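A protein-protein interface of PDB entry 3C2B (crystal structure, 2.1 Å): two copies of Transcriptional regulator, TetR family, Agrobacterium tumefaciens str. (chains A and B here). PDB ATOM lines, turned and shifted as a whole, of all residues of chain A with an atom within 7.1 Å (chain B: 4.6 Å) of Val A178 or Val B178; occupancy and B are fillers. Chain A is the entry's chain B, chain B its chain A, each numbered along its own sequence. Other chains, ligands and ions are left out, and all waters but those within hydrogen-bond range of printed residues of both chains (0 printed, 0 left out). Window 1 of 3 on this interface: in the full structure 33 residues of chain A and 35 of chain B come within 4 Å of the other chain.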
ATOM      1  N   ASN A 113      33.048  -1.376 -13.158  1.00  0.00           N
ATOM      2  CA  ASN A 113      31.797  -1.385 -13.878  1.00  0.00           C
ATOM      3  C   ASN A 113      30.818  -2.365 -13.254  1.00  0.00           C
ATOM      4  O   ASN A 113      29.652  -2.065 -13.161  1.00  0.00           O
ATOM      5  CB  ASN A 113      32.031  -1.733 -15.335  1.00  0.00           C
ATOM      6  CG  ASN A 113      32.457  -0.558 -16.137  1.00  0.00           C
ATOM      7  OD1 ASN A 113      31.634   0.277 -16.501  1.00  0.00           O
ATOM      8  ND2 ASN A 113      33.734  -0.513 -16.485  1.00  0.00           N
ATOM      9  N   ILE A 117      27.342  -1.053 -11.880  1.00  0.00           N
ATOM     10  CA  ILE A 117      26.177  -1.651 -12.480  1.00  0.00           C
ATOM     11  C   ILE A 117      25.409  -2.509 -11.479  1.00  0.00           C
ATOM     12  O   ILE A 117      24.182  -2.455 -11.454  1.00  0.00           O
ATOM     13  CB  ILE A 117      26.553  -2.471 -13.717  1.00  0.00           C
ATOM     14  CG1 ILE A 117      27.009  -1.506 -14.828  1.00  0.00           C
ATOM     15  CG2 ILE A 117      25.365  -3.377 -14.149  1.00  0.00           C
ATOM     16  CD1 ILE A 117      27.532  -2.190 -16.084  1.00  0.00           C
ATOM     17  N   LEU A 132      30.073   7.207 -16.142  1.00  0.00           N
ATOM     18  CA  LEU A 132      29.423   7.802 -17.337  1.00  0.00           C
ATOM     19  C   LEU A 132      30.119   9.132 -17.677  1.00  0.00           C
ATOM     20  O   LEU A 132      30.284   9.484 -18.850  1.00  0.00           O
ATOM     21  CB  LEU A 132      27.932   8.044 -17.040  1.00  0.00           C
ATOM     22  CG  LEU A 132      26.736   7.219 -17.557  1.00  0.00           C
ATOM     23  CD1 LEU A 132      27.043   6.065 -18.545  1.00  0.00           C
ATOM     24  CD2 LEU A 132      25.787   6.796 -16.435  1.00  0.00           C
ATOM     25  N   ARG A 136      36.066   6.847 -19.174  1.00  0.00           N
ATOM     26  CA  ARG A 136      36.798   6.529 -20.379  1.00  0.00           C
ATOM     27  C   ARG A 136      37.351   7.788 -21.026  1.00  0.00           C
ATOM     28  O   ARG A 136      37.493   7.863 -22.248  1.00  0.00           O
ATOM     29  CB  ARG A 136      35.861   5.782 -21.350  1.00  0.00           C
ATOM     30  CG  ARG A 136      36.471   4.489 -21.943  1.00  0.00           C
ATOM     31  CD  ARG A 136      35.479   3.825 -22.990  1.00  0.00           C
ATOM     32  NE  ARG A 136      34.788   4.794 -23.859  1.00  0.00           N
ATOM     33  CZ  ARG A 136      33.463   4.839 -24.045  1.00  0.00           C
ATOM     34  NH1 ARG A 136      32.682   3.925 -23.468  1.00  0.00           N
ATOM     35  NH2 ARG A 136      32.917   5.745 -24.858  1.00  0.00           N
ATOM     36  N   TYR A 169      33.566   2.284 -32.182  1.00  0.00           N
ATOM     37  CA  TYR A 169      33.448   1.575 -30.912  1.00  0.00           C
ATOM     38  C   TYR A 169      32.556   0.321 -31.014  1.00  0.00           C
ATOM     39  O   TYR A 169      32.901  -0.785 -30.490  1.00  0.00           O
ATOM     40  CB  TYR A 169      32.897   2.565 -29.831  1.00  0.00           C
ATOM     41  CG  TYR A 169      33.006   2.078 -28.407  1.00  0.00           C
ATOM     42  CD1 TYR A 169      32.132   1.119 -27.910  1.00  0.00           C
ATOM     43  CD2 TYR A 169      34.008   2.583 -27.544  1.00  0.00           C
ATOM     44  CE1 TYR A 169      32.246   0.676 -26.578  1.00  0.00           C
ATOM     45  CE2 TYR A 169      34.114   2.127 -26.181  1.00  0.00           C
ATOM     46  CZ  TYR A 169      33.236   1.174 -25.742  1.00  0.00           C
ATOM     47  OH  TYR A 169      33.313   0.692 -24.423  1.00  0.00           O
ATOM     48  N   VAL A 173      33.934  -3.488 -30.341  1.00  0.00           N
ATOM     49  CA  VAL A 173      33.420  -4.120 -29.118  1.00  0.00           C
ATOM     50  C   VAL A 173      32.179  -4.975 -29.295  1.00  0.00           C
ATOM     51  O   VAL A 173      32.071  -6.043 -28.672  1.00  0.00           O
ATOM     52  CB  VAL A 173      33.104  -3.054 -28.016  1.00  0.00           C
ATOM     53  CG1 VAL A 173      32.718  -3.732 -26.668  1.00  0.00           C
ATOM     54  CG2 VAL A 173      34.328  -2.169 -27.780  1.00  0.00           C
ATOM     55  N   SER A 174      31.244  -4.507 -30.130  1.00  0.00           N
ATOM     56  CA  SER A 174      29.934  -5.154 -30.208  1.00  0.00           C
ATOM     57  C   SER A 174      29.405  -5.429 -28.779  1.00  0.00           C
ATOM     58  O   SER A 174      29.419  -4.526 -27.937  1.00  0.00           O
ATOM     59  CB  SER A 174      30.035  -6.414 -31.110  1.00  0.00           C
ATOM     60  OG  SER A 174      28.776  -6.864 -31.578  1.00  0.00           O
ATOM     61  N   ASP A 175      28.974  -6.657 -28.474  1.00  0.00           N
ATOM     62  CA  ASP A 175      28.403  -6.907 -27.180  1.00  0.00           C
ATOM     63  C   ASP A 175      29.401  -7.511 -26.221  1.00  0.00           C
ATOM     64  O   ASP A 175      29.003  -8.004 -25.198  1.00  0.00           O
ATOM     65  CB  ASP A 175      27.172  -7.802 -27.309  1.00  0.00           C
ATOM     66  CG  ASP A 175      27.516  -9.194 -27.839  1.00  0.00           C
ATOM     67  OD1 ASP A 175      28.563  -9.396 -28.477  1.00  0.00           O
ATOM     68  OD2 ASP A 175      26.738 -10.115 -27.581  1.00  0.00           O
ATOM     69  N   LEU A 176      30.690  -7.447 -26.545  1.00  0.00           N
ATOM     70  CA  LEU A 176      31.730  -8.102 -25.750  1.00  0.00           C
ATOM     71  C   LEU A 176      31.860  -7.544 -24.342  1.00  0.00           C
ATOM     72  O   LEU A 176      32.087  -8.324 -23.383  1.00  0.00           O
ATOM     73  CB  LEU A 176      33.093  -8.062 -26.445  1.00  0.00           C
ATOM     74  CG  LEU A 176      34.228  -8.900 -25.791  1.00  0.00           C
ATOM     75  CD1 LEU A 176      33.906 -10.404 -25.654  1.00  0.00           C
ATOM     76  CD2 LEU A 176      35.557  -8.689 -26.537  1.00  0.00           C
ATOM     77  N   HIS A 177      31.732  -6.218 -24.201  1.00  0.00           N
ATOM     78  CA  HIS A 177      31.805  -5.617 -22.859  1.00  0.00           C
ATOM     79  C   HIS A 177      30.733  -6.165 -21.923  1.00  0.00           C
ATOM     80  O   HIS A 177      31.050  -6.671 -20.871  1.00  0.00           O
ATOM     81  CB  HIS A 177      31.784  -4.069 -22.885  1.00  0.00           C
ATOM     82  CG  HIS A 177      32.261  -3.450 -21.608  1.00  0.00           C
ATOM     83  ND1 HIS A 177      32.028  -2.130 -21.272  1.00  0.00           N
ATOM     84  CD2 HIS A 177      32.971  -3.979 -20.579  1.00  0.00           C
ATOM     85  CE1 HIS A 177      32.579  -1.877 -20.099  1.00  0.00           C
ATOM     86  NE2 HIS A 177      33.131  -2.989 -19.645  1.00  0.00           N
ATOM     87  N   VAL A 178      29.469  -6.149 -22.348  1.00  0.00           N
ATOM     88  CA  VAL A 178      28.391  -6.737 -21.554  1.00  0.00           C
ATOM     89  C   VAL A 178      28.631  -8.218 -21.270  1.00  0.00           C
ATOM     90  O   VAL A 178      28.357  -8.698 -20.158  1.00  0.00           O
ATOM     91  CB  VAL A 178      26.975  -6.559 -22.207  1.00  0.00           C
ATOM     92  CG1 VAL A 178      25.900  -7.306 -21.397  1.00  0.00           C
ATOM     93  CG2 VAL A 178      26.599  -5.092 -22.349  1.00  0.00           C
ATOM     94  N   ARG A 179      29.105  -8.946 -22.261  1.00  0.00           N
ATOM     95  CA  ARG A 179      29.298 -10.389 -22.124  1.00  0.00           C
ATOM     96  C   ARG A 179      30.370 -10.674 -21.075  1.00  0.00           C
ATOM     97  O   ARG A 179      30.173 -11.523 -20.230  1.00  0.00           O
ATOM     98  CB  ARG A 179      29.686 -11.015 -23.477  1.00  0.00           C
ATOM     99  CG  ARG A 179      28.482 -11.319 -24.398  1.00  0.00           C
ATOM    100  CD  ARG A 179      28.933 -12.053 -25.675  1.00  0.00           C
ATOM    101  NE  ARG A 179      27.777 -12.429 -26.507  1.00  0.00           N
ATOM    102  CZ  ARG A 179      26.951 -13.461 -26.280  1.00  0.00           C
ATOM    103  NH1 ARG A 179      25.939 -13.676 -27.116  1.00  0.00           N
ATOM    104  NH2 ARG A 179      27.106 -14.279 -25.230  1.00  0.00           N
ATOM    105  N   MET A 180      31.495  -9.962 -21.142  1.00  0.00           N
ATOM    106  CA  MET A 180      32.547 -10.032 -20.128  1.00  0.00           C
ATOM    107  C   MET A 180      32.082  -9.564 -18.746  1.00  0.00           C
ATOM    108  O   MET A 180      32.464 -10.138 -17.717  1.00  0.00           O
ATOM    109  CB  MET A 180      33.756  -9.207 -20.552  1.00  0.00           C
ATOM    110  CG  MET A 180      34.501  -9.737 -21.813  1.00  0.00           C
ATOM    111  SD  MET A 180      36.245  -8.997 -22.123  1.00  0.00           S
ATOM    112  CE  MET A 180      35.812  -7.132 -22.516  1.00  0.00           C
ATOM    113  N   LEU A 181      31.291  -8.501 -18.712  1.00  0.00           N
ATOM    114  CA  LEU A 181      30.676  -8.032 -17.449  1.00  0.00           C
ATOM    115  C   LEU A 181      29.868  -9.157 -16.821  1.00  0.00           C
ATOM    116  O   LEU A 181      29.807  -9.282 -15.610  1.00  0.00           O
ATOM    117  CB  LEU A 181      29.762  -6.824 -17.721  1.00  0.00           C
ATOM    118  CG  LEU A 181      30.257  -5.389 -17.457  1.00  0.00           C
ATOM    119  CD1 LEU A 181      31.684  -5.246 -16.899  1.00  0.00           C
ATOM    120  CD2 LEU A 181      29.909  -4.374 -18.554  1.00  0.00           C
ATOM    121  N   LEU A 182      29.260  -9.984 -17.655  1.00  0.00           N
ATOM    122  CA  LEU A 182      28.447 -11.088 -17.174  1.00  0.00           C
ATOM    123  C   LEU A 182      29.245 -12.356 -16.901  1.00  0.00           C
ATOM    124  O   LEU A 182      28.696 -13.318 -16.452  1.00  0.00           O
ATOM    125  CB  LEU A 182      27.327 -11.401 -18.170  1.00  0.00           C
ATOM    126  CG  LEU A 182      26.130 -10.453 -18.305  1.00  0.00           C
ATOM    127  CD1 LEU A 182      25.449 -10.625 -19.661  1.00  0.00           C
ATOM    128  CD2 LEU A 182      25.136 -10.700 -17.146  1.00  0.00           C
ATOM    129  N   GLY A 183      30.527 -12.376 -17.225  1.00  0.00           N
ATOM    130  CA  GLY A 183      31.396 -13.458 -16.782  1.00  0.00           C
ATOM    131  C   GLY A 183      32.025 -14.261 -17.876  1.00  0.00           C
ATOM    132  O   GLY A 183      32.767 -15.211 -17.602  1.00  0.00           O
ATOM    133  N   GLU A 184      31.746 -13.887 -19.115  1.00  0.00           N
ATOM    134  CA  GLU A 184      32.363 -14.543 -20.240  1.00  0.00           C
ATOM    135  C   GLU A 184      33.849 -14.152 -20.336  1.00  0.00           C
ATOM    136  O   GLU A 184      34.212 -12.984 -20.170  1.00  0.00           O
ATOM    137  CB  GLU A 184      31.599 -14.192 -21.512  1.00  0.00           C
ATOM    138  CG  GLU A 184      32.037 -14.953 -22.784  1.00  0.00           C
ATOM    139  CD  GLU A 184      31.112 -14.689 -23.965  1.00  0.00           C
ATOM    140  OE1 GLU A 184      29.889 -14.953 -23.858  1.00  0.00           O
ATOM    141  OE2 GLU A 184      31.603 -14.207 -24.993  1.00  0.00           O
ATOM    142  N   ASP B 175      27.963   1.510 -27.360  1.00  0.00           N
ATOM    143  CA  ASP B 175      28.069   1.319 -25.898  1.00  0.00           C
ATOM    144  C   ASP B 175      26.746   1.619 -25.164  1.00  0.00           C
ATOM    145  O   ASP B 175      26.734   1.755 -23.968  1.00  0.00           O
ATOM    146  CB  ASP B 175      29.213   2.179 -25.315  1.00  0.00           C
ATOM    147  CG  ASP B 175      28.965   3.659 -25.531  1.00  0.00           C
ATOM    148  OD1 ASP B 175      28.187   4.040 -26.445  1.00  0.00           O
ATOM    149  OD2 ASP B 175      29.551   4.448 -24.804  1.00  0.00           O
ATOM    150  N   LEU B 176      25.624   1.717 -25.878  1.00  0.00           N
ATOM    151  CA  LEU B 176      24.430   2.195 -25.222  1.00  0.00           C
ATOM    152  C   LEU B 176      23.900   1.256 -24.142  1.00  0.00           C
ATOM    153  O   LEU B 176      23.281   1.709 -23.187  1.00  0.00           O
ATOM    154  CB  LEU B 176      23.345   2.479 -26.265  1.00  0.00           C
ATOM    155  CG  LEU B 176      22.046   2.994 -25.669  1.00  0.00           C
ATOM    156  CD1 LEU B 176      22.194   4.448 -25.115  1.00  0.00           C
ATOM    157  CD2 LEU B 176      20.950   2.889 -26.693  1.00  0.00           C
ATOM    158  N   HIS B 177      24.100  -0.062 -24.302  1.00  0.00           N
ATOM    159  CA  HIS B 177      23.580  -1.010 -23.304  1.00  0.00           C
ATOM    160  C   HIS B 177      24.319  -0.841 -21.968  1.00  0.00           C
ATOM    161  O   HIS B 177      23.672  -0.654 -20.932  1.00  0.00           O
ATOM    162  CB  HIS B 177      23.643  -2.460 -23.830  1.00  0.00           C
ATOM    163  CG  HIS B 177      22.885  -3.435 -22.998  1.00  0.00           C
ATOM    164  ND1 HIS B 177      23.080  -4.794 -23.085  1.00  0.00           N
ATOM    165  CD2 HIS B 177      21.877  -3.255 -22.101  1.00  0.00           C
ATOM    166  CE1 HIS B 177      22.220  -5.414 -22.278  1.00  0.00           C
ATOM    167  NE2 HIS B 177      21.496  -4.500 -21.656  1.00  0.00           N
ATOM    168  N   VAL B 178      25.654  -0.867 -22.003  1.00  0.00           N
ATOM    169  CA  VAL B 178      26.504  -0.469 -20.858  1.00  0.00           C
ATOM    170  C   VAL B 178      26.091   0.907 -20.233  1.00  0.00           C
ATOM    171  O   VAL B 178      25.805   0.973 -19.035  1.00  0.00           O
ATOM    172  CB  VAL B 178      28.058  -0.602 -21.157  1.00  0.00           C
ATOM    173  CG1 VAL B 178      28.889  -0.181 -19.965  1.00  0.00           C
ATOM    174  CG2 VAL B 178      28.428  -2.028 -21.497  1.00  0.00           C
ATOM    175  N   ARG B 179      25.974   1.977 -21.024  1.00  0.00           N
ATOM    176  CA  ARG B 179      25.502   3.246 -20.444  1.00  0.00           C
ATOM    177  C   ARG B 179      24.171   3.161 -19.680  1.00  0.00           C
ATOM    178  O   ARG B 179      24.030   3.761 -18.611  1.00  0.00           O
ATOM    179  CB  ARG B 179      25.464   4.359 -21.504  1.00  0.00           C
ATOM    180  CG  ARG B 179      26.863   4.524 -22.197  1.00  0.00           C
ATOM    181  CD  ARG B 179      26.961   5.717 -23.147  1.00  0.00           C
ATOM    182  NE  ARG B 179      26.827   6.986 -22.442  1.00  0.00           N
ATOM    183  CZ  ARG B 179      27.794   7.599 -21.741  1.00  0.00           C
ATOM    184  NH1 ARG B 179      27.513   8.754 -21.122  1.00  0.00           N
ATOM    185  NH2 ARG B 179      29.022   7.062 -21.625  1.00  0.00           N
ATOM    186  N   MET B 180      23.200   2.428 -20.240  1.00  0.00           N
ATOM    187  CA  MET B 180      21.872   2.323 -19.644  1.00  0.00           C
ATOM    188  C   MET B 180      21.932   1.520 -18.362  1.00  0.00           C
ATOM    189  O   MET B 180      21.293   1.866 -17.366  1.00  0.00           O
ATOM    190  CB  MET B 180      20.853   1.741 -20.635  1.00  0.00           C
ATOM    191  CG  MET B 180      20.503   2.695 -21.804  1.00  0.00           C
ATOM    192  SD  MET B 180      18.993   2.121 -22.899  1.00  0.00           S
ATOM    193  CE  MET B 180      19.688   0.451 -23.511  1.00  0.00           C
ATOM    194  N   LEU B 181      22.762   0.496 -18.381  1.00  0.00           N
ATOM    195  CA  LEU B 181      22.997  -0.363 -17.241  1.00  0.00           C
ATOM    196  C   LEU B 181      23.583   0.390 -16.082  1.00  0.00           C
ATOM    197  O   LEU B 181      23.293   0.095 -14.934  1.00  0.00           O
ATOM    198  CB  LEU B 181      23.921  -1.514 -17.640  1.00  0.00           C
ATOM    199  CG  LEU B 181      23.263  -2.612 -18.491  1.00  0.00           C
ATOM    200  CD1 LEU B 181      24.313  -3.649 -18.942  1.00  0.00           C
ATOM    201  CD2 LEU B 181      22.165  -3.284 -17.749  1.00  0.00           C
ATOM    202  N   LEU B 182      24.415   1.373 -16.404  1.00  0.00           N
ATOM    203  CA  LEU B 182      25.029   2.275 -15.432  1.00  0.00           C
ATOM    204  C   LEU B 182      23.992   3.300 -14.983  1.00  0.00           C
ATOM    205  O   LEU B 182      24.215   4.011 -14.023  1.00  0.00           O
ATOM    206  CB  LEU B 182      26.275   2.968 -16.030  1.00  0.00           C
ATOM    207  CG  LEU B 182      27.546   2.120 -16.246  1.00  0.00           C
ATOM    208  CD1 LEU B 182      28.489   2.805 -17.251  1.00  0.00           C
ATOM    209  CD2 LEU B 182      28.344   1.839 -14.928  1.00  0.00           C
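Val A178 touches two residues of chain B. Of chain A, only His A177 (3.6 Å) and Val A178 (3.7 Å) come within 4 Å of Val B178. Printed residues of chain B within 4 Å of Leu A132: Arg B179 and Leu B182. Of the printed residues of chain B, Arg A136 touches Asp B175. Of the printed residues of chain B, Tyr A169 touches Asp B175. Met B180 touches none of the printed residues of chain A. Gly A183 touches none of the printed residues of chain B. The nearest residue of chain A that does not touch Val B178 is Leu A181 (4.04 Å).
Of the 8 printed residues of chain B, 6 touch a printed residue of chain A. Hydrophobic or aromatic side chains of chain B within 4 Å of the printed part of chain A: His B177, Val B178, Leu B181 and Leu B182. Of the 17 printed residues of chain A, 7 touch a printed residue of chain B. Hydrophobic or aromatic side chains of chain A within 4 Å of the printed part of chain B: Ile A117, Leu A132, Tyr A169, His A177 and Val A178.
OD2 of Asp B175 is in salt-bridge range of NH1 of Arg A136, 3.4 Å away.
Among the printed residues, merely in contact across the chains: Asn A113 with Leu B182, Ile A117 with Leu B181, Ile A117 with Leu B182, Leu A132 with Arg B179, Leu A132 with Leu B182, Tyr A169 with Asp B175, His A177 with Val B178, Val A178 with His B177 and Val A178 with Val B178.
The side-chain hydroxyl (OH) of Tyr A169 sits at hydrogen-bond distance from the guanidinium group (NH1) of Arg A136 (3.4 Å).
His A177 touches Val B178, and with the chains exchanged Val A178 touches His B177. Val B178 touches its own counterpart, Val A178. Positions printed for both chains: 175, 176, 177, 178, 179, 180, 181 and 182.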
